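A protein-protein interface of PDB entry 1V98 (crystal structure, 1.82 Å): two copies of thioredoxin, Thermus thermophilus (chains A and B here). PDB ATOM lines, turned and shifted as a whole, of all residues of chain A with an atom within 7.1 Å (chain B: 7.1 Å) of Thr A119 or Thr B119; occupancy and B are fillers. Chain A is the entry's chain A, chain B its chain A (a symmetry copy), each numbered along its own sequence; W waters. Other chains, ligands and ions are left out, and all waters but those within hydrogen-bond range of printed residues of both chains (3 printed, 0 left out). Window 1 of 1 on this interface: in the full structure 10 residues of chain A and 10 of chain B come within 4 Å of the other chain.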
ATOM      1  N   PHE A  57     -33.644  -1.224  -3.918  1.00  0.00           N
ATOM      2  CA  PHE A  57     -34.808  -0.477  -3.452  1.00  0.00           C
ATOM      3  C   PHE A  57     -35.795  -0.500  -4.621  1.00  0.00           C
ATOM      4  O   PHE A  57     -35.499   0.012  -5.706  1.00  0.00           O
ATOM      5  CB  PHE A  57     -34.408   0.964  -3.097  1.00  0.00           C
ATOM      6  CG  PHE A  57     -33.570   1.066  -1.841  1.00  0.00           C
ATOM      7  CD1 PHE A  57     -34.171   1.142  -0.586  1.00  0.00           C
ATOM      8  CD2 PHE A  57     -32.180   1.093  -1.915  1.00  0.00           C
ATOM      9  CE1 PHE A  57     -33.393   1.219   0.573  1.00  0.00           C
ATOM     10  CE2 PHE A  57     -31.400   1.169  -0.764  1.00  0.00           C
ATOM     11  CZ  PHE A  57     -32.006   1.245   0.484  1.00  0.00           C
ATOM     12  N   TYR A 100     -31.331   6.419   3.096  1.00  0.00           N
ATOM     13  CA  TYR A 100     -30.350   6.301   2.033  1.00  0.00           C
ATOM     14  C   TYR A 100     -30.641   7.113   0.778  1.00  0.00           C
ATOM     15  O   TYR A 100     -30.135   6.796  -0.303  1.00  0.00           O
ATOM     16  CB  TYR A 100     -30.127   4.823   1.706  1.00  0.00           C
ATOM     17  CG  TYR A 100     -29.417   4.121   2.838  1.00  0.00           C
ATOM     18  CD1 TYR A 100     -28.095   4.444   3.160  1.00  0.00           C
ATOM     19  CD2 TYR A 100     -30.078   3.184   3.630  1.00  0.00           C
ATOM     20  CE1 TYR A 100     -27.452   3.851   4.240  1.00  0.00           C
ATOM     21  CE2 TYR A 100     -29.440   2.587   4.712  1.00  0.00           C
ATOM     22  CZ  TYR A 100     -28.134   2.925   5.010  1.00  0.00           C
ATOM     23  OH  TYR A 100     -27.511   2.331   6.075  1.00  0.00           O
ATOM     24  N   GLY A 101     -31.458   8.153   0.940  1.00  0.00           N
ATOM     25  CA  GLY A 101     -31.786   9.062  -0.144  1.00  0.00           C
ATOM     26  C   GLY A 101     -32.464   8.521  -1.379  1.00  0.00           C
ATOM     27  O   GLY A 101     -32.307   9.073  -2.466  1.00  0.00           O
ATOM     28  N   VAL A 102     -33.219   7.445  -1.229  1.00  0.00           N
ATOM     29  CA  VAL A 102     -33.915   6.869  -2.365  1.00  0.00           C
ATOM     30  C   VAL A 102     -35.141   7.725  -2.696  1.00  0.00           C
ATOM     31  O   VAL A 102     -36.054   7.857  -1.879  1.00  0.00           O
ATOM     32  CB  VAL A 102     -34.340   5.417  -2.051  1.00  0.00           C
ATOM     33  CG1 VAL A 102     -35.163   4.843  -3.198  1.00  0.00           C
ATOM     34  CG2 VAL A 102     -33.097   4.568  -1.802  1.00  0.00           C
ATOM     35  N   THR A 107     -33.528   1.796  -7.272  1.00  0.00           N
ATOM     36  CA  THR A 107     -32.274   2.450  -6.912  1.00  0.00           C
ATOM     37  C   THR A 107     -31.473   1.324  -6.282  1.00  0.00           C
ATOM     38  O   THR A 107     -31.969   0.602  -5.408  1.00  0.00           O
ATOM     39  CB  THR A 107     -32.446   3.608  -5.904  1.00  0.00           C
ATOM     40  OG1 THR A 107     -33.173   4.683  -6.516  1.00  0.00           O
ATOM     41  CG2 THR A 107     -31.071   4.140  -5.469  1.00  0.00           C
ATOM     42  N   LEU A 108     -30.254   1.153  -6.778  1.00  0.00           N
ATOM     43  CA  LEU A 108     -29.360   0.114  -6.294  1.00  0.00           C
ATOM     44  C   LEU A 108     -28.245   0.775  -5.493  1.00  0.00           C
ATOM     45  O   LEU A 108     -27.579   1.698  -5.975  1.00  0.00           O
ATOM     46  CB  LEU A 108     -28.759  -0.662  -7.468  1.00  0.00           C
ATOM     47  CG  LEU A 108     -29.690  -1.135  -8.590  1.00  0.00           C
ATOM     48  CD1 LEU A 108     -28.927  -2.119  -9.461  1.00  0.00           C
ATOM     49  CD2 LEU A 108     -30.950  -1.782  -8.023  1.00  0.00           C
ATOM     50  N   VAL A 109     -28.056   0.307  -4.265  1.00  0.00           N
ATOM     51  CA  VAL A 109     -27.030   0.857  -3.399  1.00  0.00           C
ATOM     52  C   VAL A 109     -26.068  -0.256  -2.978  1.00  0.00           C
ATOM     53  O   VAL A 109     -26.493  -1.285  -2.432  1.00  0.00           O
ATOM     54  CB  VAL A 109     -27.657   1.503  -2.128  1.00  0.00           C
ATOM     55  CG1 VAL A 109     -26.569   2.125  -1.280  1.00  0.00           C
ATOM     56  CG2 VAL A 109     -28.707   2.561  -2.522  1.00  0.00           C
ATOM     57  N   LEU A 110     -24.778  -0.052  -3.251  1.00  0.00           N
ATOM     58  CA  LEU A 110     -23.727  -1.015  -2.904  1.00  0.00           C
ATOM     59  C   LEU A 110     -23.084  -0.632  -1.571  1.00  0.00           C
ATOM     60  O   LEU A 110     -22.597   0.490  -1.411  1.00  0.00           O
ATOM     61  CB  LEU A 110     -22.642  -1.038  -4.002  1.00  0.00           C
ATOM     62  CG  LEU A 110     -21.471  -2.016  -3.790  1.00  0.00           C
ATOM     63  CD1 LEU A 110     -22.043  -3.418  -3.705  1.00  0.00           C
ATOM     64  CD2 LEU A 110     -20.437  -1.925  -4.922  1.00  0.00           C
ATOM     65  N   PRO A 116     -22.745   2.826   2.274  1.00  0.00           N
ATOM     66  CA  PRO A 116     -22.820   2.869   0.813  1.00  0.00           C
ATOM     67  C   PRO A 116     -21.523   3.373   0.196  1.00  0.00           C
ATOM     68  O   PRO A 116     -20.908   4.300   0.723  1.00  0.00           O
ATOM     69  CB  PRO A 116     -23.956   3.860   0.549  1.00  0.00           C
ATOM     70  CG  PRO A 116     -24.788   3.793   1.780  1.00  0.00           C
ATOM     71  CD  PRO A 116     -23.754   3.713   2.876  1.00  0.00           C
ATOM     72  N   VAL A 117     -21.092   2.755  -0.901  1.00  0.00           N
ATOM     73  CA  VAL A 117     -19.914   3.248  -1.603  1.00  0.00           C
ATOM     74  C   VAL A 117     -20.352   3.700  -2.989  1.00  0.00           C
ATOM     75  O   VAL A 117     -19.703   4.542  -3.600  1.00  0.00           O
ATOM     76  CB  VAL A 117     -18.761   2.196  -1.727  1.00  0.00           C
ATOM     77  CG1 VAL A 117     -18.166   1.930  -0.357  1.00  0.00           C
ATOM     78  CG2 VAL A 117     -19.249   0.921  -2.387  1.00  0.00           C
ATOM     79  N   ALA A 118     -21.469   3.167  -3.475  1.00  0.00           N
ATOM     80  CA  ALA A 118     -21.974   3.565  -4.792  1.00  0.00           C
ATOM     81  C   ALA A 118     -23.489   3.423  -4.841  1.00  0.00           C
ATOM     82  O   ALA A 118     -24.050   2.553  -4.175  1.00  0.00           O
ATOM     83  CB  ALA A 118     -21.339   2.707  -5.877  1.00  0.00           C
ATOM     84  N   THR A 119     -24.148   4.283  -5.615  1.00  0.00           N
ATOM     85  CA  THR A 119     -25.601   4.229  -5.772  1.00  0.00           C
ATOM     86  C   THR A 119     -25.911   4.502  -7.246  1.00  0.00           C
ATOM     87  O   THR A 119     -25.430   5.483  -7.810  1.00  0.00           O
ATOM     88  CB  THR A 119     -26.319   5.305  -4.895  1.00  0.00           C
ATOM     89  OG1 THR A 119     -26.092   5.027  -3.506  1.00  0.00           O
ATOM     90  CG2 THR A 119     -27.825   5.300  -5.167  1.00  0.00           C
ATOM     91  N   TRP A 120     -26.684   3.623  -7.877  1.00  0.00           N
ATOM     92  CA  TRP A 120     -27.048   3.813  -9.278  1.00  0.00           C
ATOM     93  C   TRP A 120     -28.564   3.903  -9.347  1.00  0.00           C
ATOM     94  O   TRP A 120     -29.270   3.064  -8.785  1.00  0.00           O
ATOM     95  CB  TRP A 120     -26.557   2.650 -10.133  1.00  0.00           C
ATOM     96  CG  TRP A 120     -25.077   2.465 -10.071  1.00  0.00           C
ATOM     97  CD1 TRP A 120     -24.133   3.142 -10.781  1.00  0.00           C
ATOM     98  CD2 TRP A 120     -24.376   1.533  -9.247  1.00  0.00           C
ATOM     99  NE1 TRP A 120     -22.878   2.683 -10.453  1.00  0.00           N
ATOM    100  CE2 TRP A 120     -23.001   1.692  -9.510  1.00  0.00           C
ATOM    101  CE3 TRP A 120     -24.779   0.572  -8.311  1.00  0.00           C
ATOM    102  CZ2 TRP A 120     -22.021   0.929  -8.871  1.00  0.00           C
ATOM    103  CZ3 TRP A 120     -23.807  -0.189  -7.676  1.00  0.00           C
ATOM    104  CH2 TRP A 120     -22.443  -0.005  -7.960  1.00  0.00           C
ATOM    105  N   VAL A 121     -29.061   4.925 -10.031  1.00  0.00           N
ATOM    106  CA  VAL A 121     -30.495   5.143 -10.130  1.00  0.00           C
ATOM    107  C   VAL A 121     -31.063   4.693 -11.467  1.00  0.00           C
ATOM    108  O   VAL A 121     -30.528   5.042 -12.522  1.00  0.00           O
ATOM    109  CB  VAL A 121     -30.808   6.644  -9.906  1.00  0.00           C
ATOM    110  CG1 VAL A 121     -32.288   6.912 -10.067  1.00  0.00           C
ATOM    111  CG2 VAL A 121     -30.340   7.065  -8.511  1.00  0.00           C
ATOM    112  N   TYR A 136     -15.536  -3.483  -7.993  1.00  0.00           N
ATOM    113  CA  TYR A 136     -15.705  -3.707  -6.555  1.00  0.00           C
ATOM    114  C   TYR A 136     -15.485  -5.187  -6.241  1.00  0.00           C
ATOM    115  O   TYR A 136     -14.880  -5.530  -5.225  1.00  0.00           O
ATOM    116  CB  TYR A 136     -17.107  -3.275  -6.109  1.00  0.00           C
ATOM    117  CG  TYR A 136     -17.369  -1.796  -6.303  1.00  0.00           C
ATOM    118  CD1 TYR A 136     -16.928  -0.862  -5.369  1.00  0.00           C
ATOM    119  CD2 TYR A 136     -18.034  -1.331  -7.436  1.00  0.00           C
ATOM    120  CE1 TYR A 136     -17.141   0.503  -5.561  1.00  0.00           C
ATOM    121  CE2 TYR A 136     -18.260   0.024  -7.637  1.00  0.00           C
ATOM    122  CZ  TYR A 136     -17.810   0.935  -6.695  1.00  0.00           C
ATOM    123  OH  TYR A 136     -18.028   2.280  -6.884  1.00  0.00           O
ATOM    124  N   PHE B  57     -18.763  17.056  -4.279  1.00  0.00           N
ATOM    125  CA  PHE B  57     -19.085  17.555  -2.945  1.00  0.00           C
ATOM    126  C   PHE B  57     -17.815  17.340  -2.119  1.00  0.00           C
ATOM    127  O   PHE B  57     -17.365  16.204  -1.938  1.00  0.00           O
ATOM    128  CB  PHE B  57     -20.266  16.767  -2.355  1.00  0.00           C
ATOM    129  CG  PHE B  57     -21.589  17.072  -3.022  1.00  0.00           C
ATOM    130  CD1 PHE B  57     -22.367  18.151  -2.608  1.00  0.00           C
ATOM    131  CD2 PHE B  57     -22.060  16.274  -4.063  1.00  0.00           C
ATOM    132  CE1 PHE B  57     -23.580  18.439  -3.238  1.00  0.00           C
ATOM    133  CE2 PHE B  57     -23.267  16.557  -4.695  1.00  0.00           C
ATOM    134  CZ  PHE B  57     -24.038  17.634  -4.276  1.00  0.00           C
ATOM    135  N   TYR B 100     -29.020  16.069  -1.671  1.00  0.00           N
ATOM    136  CA  TYR B 100     -28.507  14.936  -2.418  1.00  0.00           C
ATOM    137  C   TYR B 100     -27.869  13.833  -1.582  1.00  0.00           C
ATOM    138  O   TYR B 100     -27.062  13.050  -2.092  1.00  0.00           O
ATOM    139  CB  TYR B 100     -27.557  15.432  -3.510  1.00  0.00           C
ATOM    140  CG  TYR B 100     -28.314  16.172  -4.587  1.00  0.00           C
ATOM    141  CD1 TYR B 100     -29.218  15.499  -5.414  1.00  0.00           C
ATOM    142  CD2 TYR B 100     -28.179  17.551  -4.740  1.00  0.00           C
ATOM    143  CE1 TYR B 100     -29.967  16.181  -6.365  1.00  0.00           C
ATOM    144  CE2 TYR B 100     -28.926  18.239  -5.690  1.00  0.00           C
ATOM    145  CZ  TYR B 100     -29.814  17.550  -6.494  1.00  0.00           C
ATOM    146  OH  TYR B 100     -30.545  18.234  -7.430  1.00  0.00           O
ATOM    147  N   GLY B 101     -28.242  13.790  -0.303  1.00  0.00           N
ATOM    148  CA  GLY B 101     -27.772  12.762   0.610  1.00  0.00           C
ATOM    149  C   GLY B 101     -26.292  12.631   0.873  1.00  0.00           C
ATOM    150  O   GLY B 101     -25.811  11.545   1.187  1.00  0.00           O
ATOM    151  N   VAL B 102     -25.559  13.726   0.749  1.00  0.00           N
ATOM    152  CA  VAL B 102     -24.129  13.687   0.996  1.00  0.00           C
ATOM    153  C   VAL B 102     -23.877  13.647   2.507  1.00  0.00           C
ATOM    154  O   VAL B 102     -24.234  14.579   3.228  1.00  0.00           O
ATOM    155  CB  VAL B 102     -23.444  14.921   0.368  1.00  0.00           C
ATOM    156  CG1 VAL B 102     -21.961  14.942   0.714  1.00  0.00           C
ATOM    157  CG2 VAL B 102     -23.645  14.897  -1.144  1.00  0.00           C
ATOM    158  N   THR B 107     -17.839  13.165  -2.186  1.00  0.00           N
ATOM    159  CA  THR B 107     -18.923  12.368  -2.751  1.00  0.00           C
ATOM    160  C   THR B 107     -19.104  12.975  -4.132  1.00  0.00           C
ATOM    161  O   THR B 107     -19.208  14.200  -4.280  1.00  0.00           O
ATOM    162  CB  THR B 107     -20.242  12.460  -1.953  1.00  0.00           C
ATOM    163  OG1 THR B 107     -20.075  11.853  -0.664  1.00  0.00           O
ATOM    164  CG2 THR B 107     -21.363  11.715  -2.695  1.00  0.00           C
ATOM    165  N   LEU B 108     -19.086  12.108  -5.136  1.00  0.00           N
ATOM    166  CA  LEU B 108     -19.236  12.525  -6.521  1.00  0.00           C
ATOM    167  C   LEU B 108     -20.609  12.080  -7.009  1.00  0.00           C
ATOM    168  O   LEU B 108     -20.974  10.904  -6.891  1.00  0.00           O
ATOM    169  CB  LEU B 108     -18.149  11.887  -7.391  1.00  0.00           C
ATOM    170  CG  LEU B 108     -16.698  11.924  -6.899  1.00  0.00           C
ATOM    171  CD1 LEU B 108     -15.794  11.510  -8.048  1.00  0.00           C
ATOM    172  CD2 LEU B 108     -16.325  13.313  -6.392  1.00  0.00           C
ATOM    173  N   VAL B 109     -21.369  13.027  -7.544  1.00  0.00           N
ATOM    174  CA  VAL B 109     -22.702  12.733  -8.041  1.00  0.00           C
ATOM    175  C   VAL B 109     -22.789  13.114  -9.520  1.00  0.00           C
ATOM    176  O   VAL B 109     -22.506  14.261  -9.895  1.00  0.00           O
ATOM    177  CB  VAL B 109     -23.783  13.519  -7.242  1.00  0.00           C
ATOM    178  CG1 VAL B 109     -25.162  13.140  -7.737  1.00  0.00           C
ATOM    179  CG2 VAL B 109     -23.653  13.232  -5.732  1.00  0.00           C
ATOM    180  N   LEU B 110     -23.165  12.143 -10.355  1.00  0.00           N
ATOM    181  CA  LEU B 110     -23.308  12.346 -11.801  1.00  0.00           C
ATOM    182  C   LEU B 110     -24.767  12.647 -12.145  1.00  0.00           C
ATOM    183  O   LEU B 110     -25.662  11.867 -11.811  1.00  0.00           O
ATOM    184  CB  LEU B 110     -22.857  11.082 -12.564  1.00  0.00           C
ATOM    185  CG  LEU B 110     -22.934  11.143 -14.101  1.00  0.00           C
ATOM    186  CD1 LEU B 110     -22.047  12.280 -14.568  1.00  0.00           C
ATOM    187  CD2 LEU B 110     -22.499   9.821 -14.749  1.00  0.00           C
ATOM    188  N   PRO B 116     -29.660  13.004 -10.475  1.00  0.00           N
ATOM    189  CA  PRO B 116     -28.538  12.084 -10.281  1.00  0.00           C
ATOM    190  C   PRO B 116     -28.811  10.723 -10.904  1.00  0.00           C
ATOM    191  O   PRO B 116     -29.932  10.219 -10.819  1.00  0.00           O
ATOM    192  CB  PRO B 116     -28.441  11.963  -8.759  1.00  0.00           C
ATOM    193  CG  PRO B 116     -29.040  13.230  -8.256  1.00  0.00           C
ATOM    194  CD  PRO B 116     -30.216  13.429  -9.179  1.00  0.00           C
ATOM    195  N   VAL B 117     -27.805  10.136 -11.548  1.00  0.00           N
ATOM    196  CA  VAL B 117     -27.964   8.789 -12.081  1.00  0.00           C
ATOM    197  C   VAL B 117     -26.982   7.881 -11.354  1.00  0.00           C
ATOM    198  O   VAL B 117     -27.200   6.678 -11.266  1.00  0.00           O
ATOM    199  CB  VAL B 117     -27.738   8.686 -13.627  1.00  0.00           C
ATOM    200  CG1 VAL B 117     -28.865   9.397 -14.354  1.00  0.00           C
ATOM    201  CG2 VAL B 117     -26.380   9.231 -14.022  1.00  0.00           C
ATOM    202  N   ALA B 118     -25.916   8.457 -10.806  1.00  0.00           N
ATOM    203  CA  ALA B 118     -24.934   7.659 -10.067  1.00  0.00           C
ATOM    204  C   ALA B 118     -24.262   8.508  -8.997  1.00  0.00           C
ATOM    205  O   ALA B 118     -24.104   9.715  -9.175  1.00  0.00           O
ATOM    206  CB  ALA B 118     -23.885   7.106 -11.022  1.00  0.00           C
ATOM    207  N   THR B 119     -23.882   7.881  -7.884  1.00  0.00           N
ATOM    208  CA  THR B 119     -23.198   8.579  -6.797  1.00  0.00           C
ATOM    209  C   THR B 119     -22.100   7.647  -6.276  1.00  0.00           C
ATOM    210  O   THR B 119     -22.366   6.485  -5.974  1.00  0.00           O
ATOM    211  CB  THR B 119     -24.171   8.921  -5.624  1.00  0.00           C
ATOM    212  OG1 THR B 119     -25.170   9.846  -6.078  1.00  0.00           O
ATOM    213  CG2 THR B 119     -23.406   9.546  -4.456  1.00  0.00           C
ATOM    214  N   TRP B 120     -20.869   8.141  -6.201  1.00  0.00           N
ATOM    215  CA  TRP B 120     -19.764   7.330  -5.698  1.00  0.00           C
ATOM    216  C   TRP B 120     -19.199   8.038  -4.477  1.00  0.00           C
ATOM    217  O   TRP B 120     -18.925   9.238  -4.516  1.00  0.00           O
ATOM    218  CB  TRP B 120     -18.676   7.170  -6.754  1.00  0.00           C
ATOM    219  CG  TRP B 120     -19.172   6.532  -8.009  1.00  0.00           C
ATOM    220  CD1 TRP B 120     -19.335   5.200  -8.245  1.00  0.00           C
ATOM    221  CD2 TRP B 120     -19.568   7.207  -9.203  1.00  0.00           C
ATOM    222  NE1 TRP B 120     -19.807   5.002  -9.523  1.00  0.00           N
ATOM    223  CE2 TRP B 120     -19.958   6.223 -10.133  1.00  0.00           C
ATOM    224  CE3 TRP B 120     -19.626   8.555  -9.580  1.00  0.00           C
ATOM    225  CZ2 TRP B 120     -20.405   6.540 -11.418  1.00  0.00           C
ATOM    226  CZ3 TRP B 120     -20.068   8.872 -10.857  1.00  0.00           C
ATOM    227  CH2 TRP B 120     -20.452   7.865 -11.761  1.00  0.00           C
ATOM    228  N   VAL B 121     -19.033   7.294  -3.391  1.00  0.00           N
ATOM    229  CA  VAL B 121     -18.543   7.866  -2.148  1.00  0.00           C
ATOM    230  C   VAL B 121     -17.074   7.561  -1.903  1.00  0.00           C
ATOM    231  O   VAL B 121     -16.650   6.408  -2.010  1.00  0.00           O
ATOM    232  CB  VAL B 121     -19.393   7.340  -0.964  1.00  0.00           C
ATOM    233  CG1 VAL B 121     -18.866   7.869   0.351  1.00  0.00           C
ATOM    234  CG2 VAL B 121     -20.855   7.752  -1.155  1.00  0.00           C
ATOM    235  N   TYR B 136     -21.136   6.130 -19.266  1.00  0.00           N
ATOM    236  CA  TYR B 136     -22.054   7.266 -19.387  1.00  0.00           C
ATOM    237  C   TYR B 136     -21.593   8.175 -20.526  1.00  0.00           C
ATOM    238  O   TYR B 136     -22.412   8.696 -21.283  1.00  0.00           O
ATOM    239  CB  TYR B 136     -22.106   8.052 -18.072  1.00  0.00           C
ATOM    240  CG  TYR B 136     -22.644   7.242 -16.909  1.00  0.00           C
ATOM    241  CD1 TYR B 136     -24.014   7.087 -16.717  1.00  0.00           C
ATOM    242  CD2 TYR B 136     -21.778   6.609 -16.019  1.00  0.00           C
ATOM    243  CE1 TYR B 136     -24.511   6.317 -15.666  1.00  0.00           C
ATOM    244  CE2 TYR B 136     -22.257   5.846 -14.964  1.00  0.00           C
ATOM    245  CZ  TYR B 136     -23.625   5.703 -14.794  1.00  0.00           C
ATOM    246  OH  TYR B 136     -24.111   4.949 -13.752  1.00  0.00           O
HETATM  247  O   HOH W   1     -20.140   2.835 -11.442  1.00  0.00           O
HETATM  248  O   HOH W   2     -23.661   5.993  -2.854  1.00  0.00           O
HETATM  249  O   HOH W   3     -27.077   8.440  -7.366  1.00  0.00           O
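Among the printed residues, merely in contact across the chains: Pro A116 with Val B121, Val A117 with Trp B120, Ala A118 with Thr B119, Ala A118 with Trp B120, Thr A119 with Ala B118, Trp A120 with Val B117, Trp A120 with Ala B118, Trp A120 with Trp B120, Trp A120 with Tyr B136, Val A121 with Pro B116 and Tyr A136 with Trp B120.
N of Thr A119 lies within hydrogen-bond range of O of Thr B119.
The backbone NH (N) of Val B121 lies within hydrogen-bond range of the backbone carbonyl oxygen (O) of Val A117.
The backbone NH of Val A121 lies within hydrogen-bond range of the backbone carbonyl oxygen of Val B117, 2.8 Å away.
Water W3 lies within hydrogen-bond range of OG1 of Thr B119 (2.7 Å) and O of Thr A119 (3.4 Å).
Water W2 bridges the side-chain hydroxyl (OG1) of Thr A119 (2.7 Å) and the backbone carbonyl oxygen (O) of Thr B119 (3.4 Å).
Water W1 lies within hydrogen-bond range of NE1 of Trp B120 (2.9 Å) and NE1 of Trp A120 (2.9 Å).
Of the printed residues of chain B, Pro A116 touches Val B121 (3.8 Å).
Of the printed residues of chain B, Ala A118 touches Thr B119 (3.2 Å) and Trp B120 (3.98 Å).
Of the printed residues of chain A, Pro B116 touches Val A121.
Of chain A, only Ala A118 and Thr A119 come within 4 Å of Thr B119.
The nearest residue of chain A that does not touch Thr B119 is Val A117 (4.1 Å).
The nearest printed residue of chain A that does not touch Trp B120 is Thr A119 (5.1 Å).
Along chain A the printed residues that touch a printed residue of chain B span positions 116 to 136.
Of the 15 printed residues of chain B, 7 touch a printed residue of chain A.
Printed residues of chain B that touch a printed residue of chain A: Pro B116, Val B117, Ala B118, Thr B119, Trp B120, Val B121 and Tyr B136.
Among the printed residues, 14 pairs touch across the chains.
Among the printed residues, no Asp or Glu carboxylate lies within 4 Å of a Lys or Arg side-chain nitrogen of the other chain.
The backbone carbonyl oxygen (O) of Leu B108 sits at hydrogen-bond distance from the backbone NH (N) of Trp B120 (2.8 Å).
N of Trp A120 lies within hydrogen-bond range of O of Leu A108 (2.9 Å).
N of Leu B110 lies within hydrogen-bond range of O of Ala B118 (2.9 Å).
The backbone carbonyl oxygen of Leu A110 lies within hydrogen-bond range of the backbone NH of Val A117 (2.8 Å).
The backbone carbonyl oxygen (O) of Leu B110 lies within hydrogen-bond range of the backbone NH (N) of Val B117 (2.8 Å).
N of Leu A110 lies within hydrogen-bond range of O of Ala A118 (2.9 Å).
Ala A118 touches Thr B119, and with the chains exchanged Thr A119 touches Ala B118.
Thr B119 touches its own counterpart, Thr A119.
Trp A120 touches its own counterpart, Trp B120.
Trp A120 touches Tyr B136, and with the chains exchanged Tyr A136 touches Trp B120.
15 positions are printed for both chains.
Of the 14 pairs that touch across the chains among the printed residues, 14 have their exchanged pair printed and touching as well.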
